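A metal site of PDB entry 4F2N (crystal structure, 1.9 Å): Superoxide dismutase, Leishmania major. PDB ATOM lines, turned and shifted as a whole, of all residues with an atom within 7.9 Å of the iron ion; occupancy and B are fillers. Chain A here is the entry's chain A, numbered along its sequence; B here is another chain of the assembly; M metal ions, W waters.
Within 4 Å of the iron ion: His 58, His 108, Asp 191 and His 195.
Water W1 bridges OD1 of Asp 191 (2.8 Å) and NE2 of Gln 104 (3.3 Å).
OD2 of Asp 191 is bound to the iron ion, at 1.9 Å. NE2 of His 108 binds the iron ion, 2.1 Å away. The iron ion is bound by NE2 of His 58. The iron ion is bound by NE2 of His 195 (2.2 Å). Water W1 is bound to the iron ion. The iron ion has five donor atoms within binding distance.
The side-chain carboxylate (OD1) of Asp 191 is in hydrogen-bond range of the backbone NH (N) of Trp 193, at 3.2 Å. O of Asp 191 sits at hydrogen-bond distance from OH of Tyr 208 (2.7 Å). ND1 of His 108 is in hydrogen-bond range of O of Gln 104 (2.7 Å). The backbone carbonyl oxygen of His 108 sits close to the indole nitrogen of Trp 112 (3.5 Å). The backbone carbonyl oxygen (O) of His 58 sits at hydrogen-bond distance from the backbone NH (N) of His 63 (2.9 Å). ND1 of His 195 lies within hydrogen-bond range of OE2 of Glu 194 of chain B (2.8 Å).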
ATOM      1  N   HIS A  58     -22.528  -4.831  21.125  1.00  0.00           N
ATOM      2  CA  HIS A  58     -23.124  -4.503  19.824  1.00  0.00           C
ATOM      3  C   HIS A  58     -22.107  -4.676  18.721  1.00  0.00           C
ATOM      4  O   HIS A  58     -22.423  -5.230  17.669  1.00  0.00           O
ATOM      5  CB  HIS A  58     -23.639  -3.081  19.839  1.00  0.00           C
ATOM      6  CG  HIS A  58     -24.717  -2.823  18.794  1.00  0.00           C
ATOM      7  ND1 HIS A  58     -25.429  -1.690  18.771  1.00  0.00           N
ATOM      8  CD2 HIS A  58     -25.149  -3.590  17.718  1.00  0.00           C
ATOM      9  CE1 HIS A  58     -26.314  -1.723  17.712  1.00  0.00           C
ATOM     10  NE2 HIS A  58     -26.123  -2.891  17.064  1.00  0.00           N
ATOM     11  N   TYR A  59     -20.874  -4.227  18.974  1.00  0.00           N
ATOM     12  CA  TYR A  59     -19.804  -4.277  17.996  1.00  0.00           C
ATOM     13  C   TYR A  59     -19.100  -5.617  18.024  1.00  0.00           C
ATOM     14  O   TYR A  59     -18.991  -6.270  16.996  1.00  0.00           O
ATOM     15  CB  TYR A  59     -18.824  -3.135  18.281  1.00  0.00           C
ATOM     16  CG  TYR A  59     -17.574  -3.033  17.405  1.00  0.00           C
ATOM     17  CD1 TYR A  59     -17.609  -2.412  16.143  1.00  0.00           C
ATOM     18  CD2 TYR A  59     -16.341  -3.439  17.897  1.00  0.00           C
ATOM     19  CE1 TYR A  59     -16.449  -2.267  15.373  1.00  0.00           C
ATOM     20  CE2 TYR A  59     -15.179  -3.298  17.135  1.00  0.00           C
ATOM     21  CZ  TYR A  59     -15.244  -2.711  15.876  1.00  0.00           C
ATOM     22  OH  TYR A  59     -14.086  -2.574  15.159  1.00  0.00           O
ATOM     23  N   HIS A  62     -22.607  -8.744  18.090  1.00  0.00           N
ATOM     24  CA  HIS A  62     -23.600  -8.663  17.025  1.00  0.00           C
ATOM     25  C   HIS A  62     -22.956  -8.358  15.700  1.00  0.00           C
ATOM     26  O   HIS A  62     -23.057  -9.172  14.758  1.00  0.00           O
ATOM     27  CB  HIS A  62     -24.712  -7.642  17.374  1.00  0.00           C
ATOM     28  CG  HIS A  62     -25.547  -8.054  18.553  1.00  0.00           C
ATOM     29  ND1 HIS A  62     -26.563  -8.955  18.454  1.00  0.00           N
ATOM     30  CD2 HIS A  62     -25.466  -7.704  19.896  1.00  0.00           C
ATOM     31  CE1 HIS A  62     -27.124  -9.111  19.667  1.00  0.00           C
ATOM     32  NE2 HIS A  62     -26.449  -8.365  20.536  1.00  0.00           N
ATOM     33  N   HIS A  63     -22.280  -7.213  15.569  1.00  0.00           N
ATOM     34  CA  HIS A  63     -21.684  -6.827  14.285  1.00  0.00           C
ATOM     35  C   HIS A  63     -20.643  -7.827  13.841  1.00  0.00           C
ATOM     36  O   HIS A  63     -20.647  -8.267  12.696  1.00  0.00           O
ATOM     37  CB  HIS A  63     -21.081  -5.423  14.370  1.00  0.00           C
ATOM     38  CG  HIS A  63     -20.730  -4.799  13.020  1.00  0.00           C
ATOM     39  ND1 HIS A  63     -20.264  -3.546  12.899  1.00  0.00           N
ATOM     40  CD2 HIS A  63     -20.807  -5.316  11.722  1.00  0.00           C
ATOM     41  CE1 HIS A  63     -20.057  -3.248  11.582  1.00  0.00           C
ATOM     42  NE2 HIS A  63     -20.382  -4.344  10.865  1.00  0.00           N
ATOM     43  N   TYR A  66     -22.107 -10.932  12.061  1.00  0.00           N
ATOM     44  CA  TYR A  66     -22.494 -10.643  10.670  1.00  0.00           C
ATOM     45  C   TYR A  66     -21.266 -10.699   9.747  1.00  0.00           C
ATOM     46  O   TYR A  66     -21.336 -11.286   8.676  1.00  0.00           O
ATOM     47  CB  TYR A  66     -23.185  -9.279  10.547  1.00  0.00           C
ATOM     48  CG  TYR A  66     -24.519  -9.208  11.243  1.00  0.00           C
ATOM     49  CD1 TYR A  66     -25.572 -10.107  10.914  1.00  0.00           C
ATOM     50  CD2 TYR A  66     -24.762  -8.240  12.211  1.00  0.00           C
ATOM     51  CE1 TYR A  66     -26.793 -10.036  11.567  1.00  0.00           C
ATOM     52  CE2 TYR A  66     -25.979  -8.152  12.859  1.00  0.00           C
ATOM     53  CZ  TYR A  66     -26.987  -9.055  12.538  1.00  0.00           C
ATOM     54  OH  TYR A  66     -28.204  -8.938  13.177  1.00  0.00           O
ATOM     55  N   GLN A 104     -26.828  -6.222   7.091  1.00  0.00           N
ATOM     56  CA  GLN A 104     -26.551  -5.898   8.479  1.00  0.00           C
ATOM     57  C   GLN A 104     -25.128  -5.339   8.685  1.00  0.00           C
ATOM     58  O   GLN A 104     -24.916  -4.475   9.539  1.00  0.00           O
ATOM     59  CB  GLN A 104     -26.812  -7.081   9.438  1.00  0.00           C
ATOM     60  CG  GLN A 104     -28.289  -7.337   9.672  1.00  0.00           C
ATOM     61  CD  GLN A 104     -28.977  -6.188  10.420  1.00  0.00           C
ATOM     62  OE1 GLN A 104     -29.356  -5.169   9.819  1.00  0.00           O
ATOM     63  NE2 GLN A 104     -29.144  -6.341  11.715  1.00  0.00           N
ATOM     64  N   ASN A 107     -25.349  -1.795   7.396  1.00  0.00           N
ATOM     65  CA  ASN A 107     -26.181  -0.968   8.293  1.00  0.00           C
ATOM     66  C   ASN A 107     -25.393  -0.609   9.562  1.00  0.00           C
ATOM     67  O   ASN A 107     -25.371   0.557   9.998  1.00  0.00           O
ATOM     68  CB  ASN A 107     -27.502  -1.688   8.669  1.00  0.00           C
ATOM     69  CG  ASN A 107     -28.435  -1.886   7.498  1.00  0.00           C
ATOM     70  OD1 ASN A 107     -28.337  -1.211   6.465  1.00  0.00           O
ATOM     71  ND2 ASN A 107     -29.374  -2.837   7.651  1.00  0.00           N
ATOM     72  N   HIS A 108     -24.709  -1.591  10.138  1.00  0.00           N
ATOM     73  CA  HIS A 108     -23.941  -1.308  11.364  1.00  0.00           C
ATOM     74  C   HIS A 108     -22.727  -0.442  11.091  1.00  0.00           C
ATOM     75  O   HIS A 108     -22.443   0.462  11.851  1.00  0.00           O
ATOM     76  CB  HIS A 108     -23.505  -2.597  12.070  1.00  0.00           C
ATOM     77  CG  HIS A 108     -24.637  -3.292  12.794  1.00  0.00           C
ATOM     78  ND1 HIS A 108     -25.443  -4.184  12.190  1.00  0.00           N
ATOM     79  CD2 HIS A 108     -25.058  -3.215  14.115  1.00  0.00           C
ATOM     80  CE1 HIS A 108     -26.365  -4.627  13.046  1.00  0.00           C
ATOM     81  NE2 HIS A 108     -26.113  -4.061  14.249  1.00  0.00           N
ATOM     82  N   PHE A 111     -24.056   2.982  10.742  1.00  0.00           N
ATOM     83  CA  PHE A 111     -24.394   3.429  12.127  1.00  0.00           C
ATOM     84  C   PHE A 111     -23.175   3.975  12.868  1.00  0.00           C
ATOM     85  O   PHE A 111     -23.228   5.068  13.451  1.00  0.00           O
ATOM     86  CB  PHE A 111     -25.004   2.245  12.922  1.00  0.00           C
ATOM     87  CG  PHE A 111     -25.706   2.635  14.212  1.00  0.00           C
ATOM     88  CD1 PHE A 111     -26.514   3.774  14.312  1.00  0.00           C
ATOM     89  CD2 PHE A 111     -25.564   1.805  15.353  1.00  0.00           C
ATOM     90  CE1 PHE A 111     -27.167   4.091  15.506  1.00  0.00           C
ATOM     91  CE2 PHE A 111     -26.207   2.126  16.546  1.00  0.00           C
ATOM     92  CZ  PHE A 111     -26.996   3.267  16.630  1.00  0.00           C
ATOM     93  N   TRP A 112     -22.063   3.249  12.836  1.00  0.00           N
ATOM     94  CA  TRP A 112     -20.888   3.671  13.644  1.00  0.00           C
ATOM     95  C   TRP A 112     -20.319   4.970  13.147  1.00  0.00           C
ATOM     96  O   TRP A 112     -19.858   5.779  13.937  1.00  0.00           O
ATOM     97  CB  TRP A 112     -19.757   2.658  13.685  1.00  0.00           C
ATOM     98  CG  TRP A 112     -20.163   1.291  14.159  1.00  0.00           C
ATOM     99  CD1 TRP A 112     -19.836   0.089  13.559  1.00  0.00           C
ATOM    100  CD2 TRP A 112     -20.987   0.936  15.328  1.00  0.00           C
ATOM    101  NE1 TRP A 112     -20.402  -0.960  14.246  1.00  0.00           N
ATOM    102  CE2 TRP A 112     -21.103  -0.521  15.307  1.00  0.00           C
ATOM    103  CE3 TRP A 112     -21.650   1.658  16.332  1.00  0.00           C
ATOM    104  CZ2 TRP A 112     -21.833  -1.218  16.270  1.00  0.00           C
ATOM    105  CZ3 TRP A 112     -22.375   0.948  17.300  1.00  0.00           C
ATOM    106  CH2 TRP A 112     -22.467  -0.461  17.271  1.00  0.00           C
ATOM    107  N   GLY A 155     -35.396  -3.362  13.484  1.00  0.00           N
ATOM    108  CA  GLY A 155     -35.167  -2.673  12.225  1.00  0.00           C
ATOM    109  C   GLY A 155     -34.340  -1.411  12.405  1.00  0.00           C
ATOM    110  O   GLY A 155     -33.591  -1.299  13.358  1.00  0.00           O
ATOM    111  N   TRP A 156     -34.510  -0.477  11.461  1.00  0.00           N
ATOM    112  CA  TRP A 156     -33.682   0.728  11.349  1.00  0.00           C
ATOM    113  C   TRP A 156     -34.563   1.854  10.935  1.00  0.00           C
ATOM    114  O   TRP A 156     -35.473   1.644  10.130  1.00  0.00           O
ATOM    115  CB  TRP A 156     -32.606   0.538  10.244  1.00  0.00           C
ATOM    116  CG  TRP A 156     -31.666  -0.609  10.539  1.00  0.00           C
ATOM    117  CD1 TRP A 156     -31.901  -1.969  10.346  1.00  0.00           C
ATOM    118  CD2 TRP A 156     -30.357  -0.541  11.182  1.00  0.00           C
ATOM    119  NE1 TRP A 156     -30.831  -2.719  10.728  1.00  0.00           N
ATOM    120  CE2 TRP A 156     -29.875  -1.927  11.275  1.00  0.00           C
ATOM    121  CE3 TRP A 156     -29.541   0.506  11.606  1.00  0.00           C
ATOM    122  CZ2 TRP A 156     -28.631  -2.239  11.797  1.00  0.00           C
ATOM    123  CZ3 TRP A 156     -28.289   0.181  12.154  1.00  0.00           C
ATOM    124  CH2 TRP A 156     -27.847  -1.158  12.247  1.00  0.00           C
ATOM    125  N   ASP A 191     -30.221   2.384  14.719  1.00  0.00           N
ATOM    126  CA  ASP A 191     -30.549   0.962  14.937  1.00  0.00           C
ATOM    127  C   ASP A 191     -31.667   0.872  15.987  1.00  0.00           C
ATOM    128  O   ASP A 191     -31.524   1.389  17.094  1.00  0.00           O
ATOM    129  CB  ASP A 191     -29.261   0.271  15.457  1.00  0.00           C
ATOM    130  CG  ASP A 191     -29.330  -1.263  15.407  1.00  0.00           C
ATOM    131  OD1 ASP A 191     -30.387  -1.864  15.075  1.00  0.00           O
ATOM    132  OD2 ASP A 191     -28.286  -1.897  15.738  1.00  0.00           O
ATOM    133  N   VAL A 192     -32.791   0.227  15.676  1.00  0.00           N
ATOM    134  CA  VAL A 192     -33.839  -0.003  16.695  1.00  0.00           C
ATOM    135  C   VAL A 192     -34.094  -1.499  16.935  1.00  0.00           C
ATOM    136  O   VAL A 192     -35.089  -1.872  17.548  1.00  0.00           O
ATOM    137  CB  VAL A 192     -35.160   0.790  16.417  1.00  0.00           C
ATOM    138  CG1 VAL A 192     -34.932   2.309  16.494  1.00  0.00           C
ATOM    139  CG2 VAL A 192     -35.758   0.418  15.064  1.00  0.00           C
ATOM    140  N   TRP A 193     -33.203  -2.366  16.450  1.00  0.00           N
ATOM    141  CA  TRP A 193     -33.115  -3.688  17.090  1.00  0.00           C
ATOM    142  C   TRP A 193     -32.952  -3.462  18.567  1.00  0.00           C
ATOM    143  O   TRP A 193     -32.234  -2.565  18.970  1.00  0.00           O
ATOM    144  CB  TRP A 193     -31.924  -4.469  16.595  1.00  0.00           C
ATOM    145  CG  TRP A 193     -32.068  -5.019  15.173  1.00  0.00           C
ATOM    146  CD1 TRP A 193     -32.259  -4.305  13.978  1.00  0.00           C
ATOM    147  CD2 TRP A 193     -31.944  -6.424  14.774  1.00  0.00           C
ATOM    148  NE1 TRP A 193     -32.311  -5.172  12.904  1.00  0.00           N
ATOM    149  CE2 TRP A 193     -32.109  -6.461  13.320  1.00  0.00           C
ATOM    150  CE3 TRP A 193     -31.746  -7.618  15.479  1.00  0.00           C
ATOM    151  CZ2 TRP A 193     -32.075  -7.660  12.600  1.00  0.00           C
ATOM    152  CZ3 TRP A 193     -31.681  -8.815  14.750  1.00  0.00           C
ATOM    153  CH2 TRP A 193     -31.840  -8.828  13.341  1.00  0.00           C
ATOM    154  N   GLU A 194     -33.666  -4.251  19.367  1.00  0.00           N
ATOM    155  CA  GLU A 194     -33.614  -4.137  20.833  1.00  0.00           C
ATOM    156  C   GLU A 194     -32.217  -4.242  21.389  1.00  0.00           C
ATOM    157  O   GLU A 194     -31.908  -3.524  22.339  1.00  0.00           O
ATOM    158  CB  GLU A 194     -34.569  -5.151  21.500  1.00  0.00           C
ATOM    159  CG  GLU A 194     -36.008  -4.879  21.026  1.00  0.00           C
ATOM    160  CD  GLU A 194     -37.045  -5.810  21.631  1.00  0.00           C
ATOM    161  OE1 GLU A 194     -36.837  -7.044  21.601  1.00  0.00           O
ATOM    162  OE2 GLU A 194     -38.090  -5.309  22.109  1.00  0.00           O
ATOM    163  N   HIS A 195     -31.358  -5.083  20.799  1.00  0.00           N
ATOM    164  CA  HIS A 195     -29.951  -5.160  21.251  1.00  0.00           C
ATOM    165  C   HIS A 195     -29.192  -3.849  21.164  1.00  0.00           C
ATOM    166  O   HIS A 195     -28.205  -3.714  21.830  1.00  0.00           O
ATOM    167  CB  HIS A 195     -29.165  -6.275  20.537  1.00  0.00           C
ATOM    168  CG  HIS A 195     -28.901  -6.001  19.065  1.00  0.00           C
ATOM    169  ND1 HIS A 195     -29.331  -6.830  18.096  1.00  0.00           N
ATOM    170  CD2 HIS A 195     -28.176  -4.992  18.427  1.00  0.00           C
ATOM    171  CE1 HIS A 195     -28.944  -6.376  16.894  1.00  0.00           C
ATOM    172  NE2 HIS A 195     -28.223  -5.258  17.082  1.00  0.00           N
ATOM    173  N   ALA A 196     -29.639  -2.888  20.337  1.00  0.00           N
ATOM    174  CA  ALA A 196     -28.943  -1.597  20.190  1.00  0.00           C
ATOM    175  C   ALA A 196     -29.021  -0.750  21.477  1.00  0.00           C
ATOM    176  O   ALA A 196     -28.110   0.065  21.794  1.00  0.00           O
ATOM    177  CB  ALA A 196     -29.576  -0.788  19.009  1.00  0.00           C
ATOM    178  N   TYR A 197     -30.114  -0.941  22.217  1.00  0.00           N
ATOM    179  CA  TYR A 197     -30.345  -0.116  23.399  1.00  0.00           C
ATOM    180  C   TYR A 197     -30.667  -0.861  24.704  1.00  0.00           C
ATOM    181  O   TYR A 197     -30.719  -0.213  25.748  1.00  0.00           O
ATOM    182  CB  TYR A 197     -31.476   0.884  23.111  1.00  0.00           C
ATOM    183  CG  TYR A 197     -32.781   0.210  22.712  1.00  0.00           C
ATOM    184  CD1 TYR A 197     -33.683  -0.259  23.664  1.00  0.00           C
ATOM    185  CD2 TYR A 197     -33.143   0.125  21.361  1.00  0.00           C
ATOM    186  CE1 TYR A 197     -34.875  -0.850  23.306  1.00  0.00           C
ATOM    187  CE2 TYR A 197     -34.335  -0.475  20.976  1.00  0.00           C
ATOM    188  CZ  TYR A 197     -35.200  -0.922  21.952  1.00  0.00           C
ATOM    189  OH  TYR A 197     -36.389  -1.497  21.567  1.00  0.00           O
ATOM    190  N   TYR A 208     -34.050   6.085  24.484  1.00  0.00           N
ATOM    191  CA  TYR A 208     -32.887   5.858  23.657  1.00  0.00           C
ATOM    192  C   TYR A 208     -32.859   6.819  22.462  1.00  0.00           C
ATOM    193  O   TYR A 208     -31.863   7.508  22.234  1.00  0.00           O
ATOM    194  CB  TYR A 208     -32.896   4.388  23.196  1.00  0.00           C
ATOM    195  CG  TYR A 208     -32.075   4.044  21.974  1.00  0.00           C
ATOM    196  CD1 TYR A 208     -30.680   4.154  21.969  1.00  0.00           C
ATOM    197  CD2 TYR A 208     -32.701   3.572  20.821  1.00  0.00           C
ATOM    198  CE1 TYR A 208     -29.944   3.803  20.837  1.00  0.00           C
ATOM    199  CE2 TYR A 208     -31.985   3.190  19.692  1.00  0.00           C
ATOM    200  CZ  TYR A 208     -30.588   3.329  19.700  1.00  0.00           C
ATOM    201  OH  TYR A 208     -29.852   2.978  18.568  1.00  0.00           O
ATOM    202  N   GLU B 194     -35.626 -10.154  21.137  1.00  0.00           N
ATOM    203  CA  GLU B 194     -34.400 -10.014  21.942  1.00  0.00           C
ATOM    204  C   GLU B 194     -34.705  -9.614  23.364  1.00  0.00           C
ATOM    205  O   GLU B 194     -33.978 -10.001  24.298  1.00  0.00           O
ATOM    206  CB  GLU B 194     -33.408  -9.031  21.307  1.00  0.00           C
ATOM    207  CG  GLU B 194     -32.809  -9.553  20.005  1.00  0.00           C
ATOM    208  CD  GLU B 194     -31.829  -8.573  19.348  1.00  0.00           C
ATOM    209  OE1 GLU B 194     -32.209  -7.390  19.104  1.00  0.00           O
ATOM    210  OE2 GLU B 194     -30.697  -9.031  19.027  1.00  0.00           O
HETATM  211 FE    FE M   1     -27.579  -3.700  15.700  1.00  0.00          FE
HETATM  212  O   HOH W   1     -29.212  -4.326  14.316  1.00  0.00           O
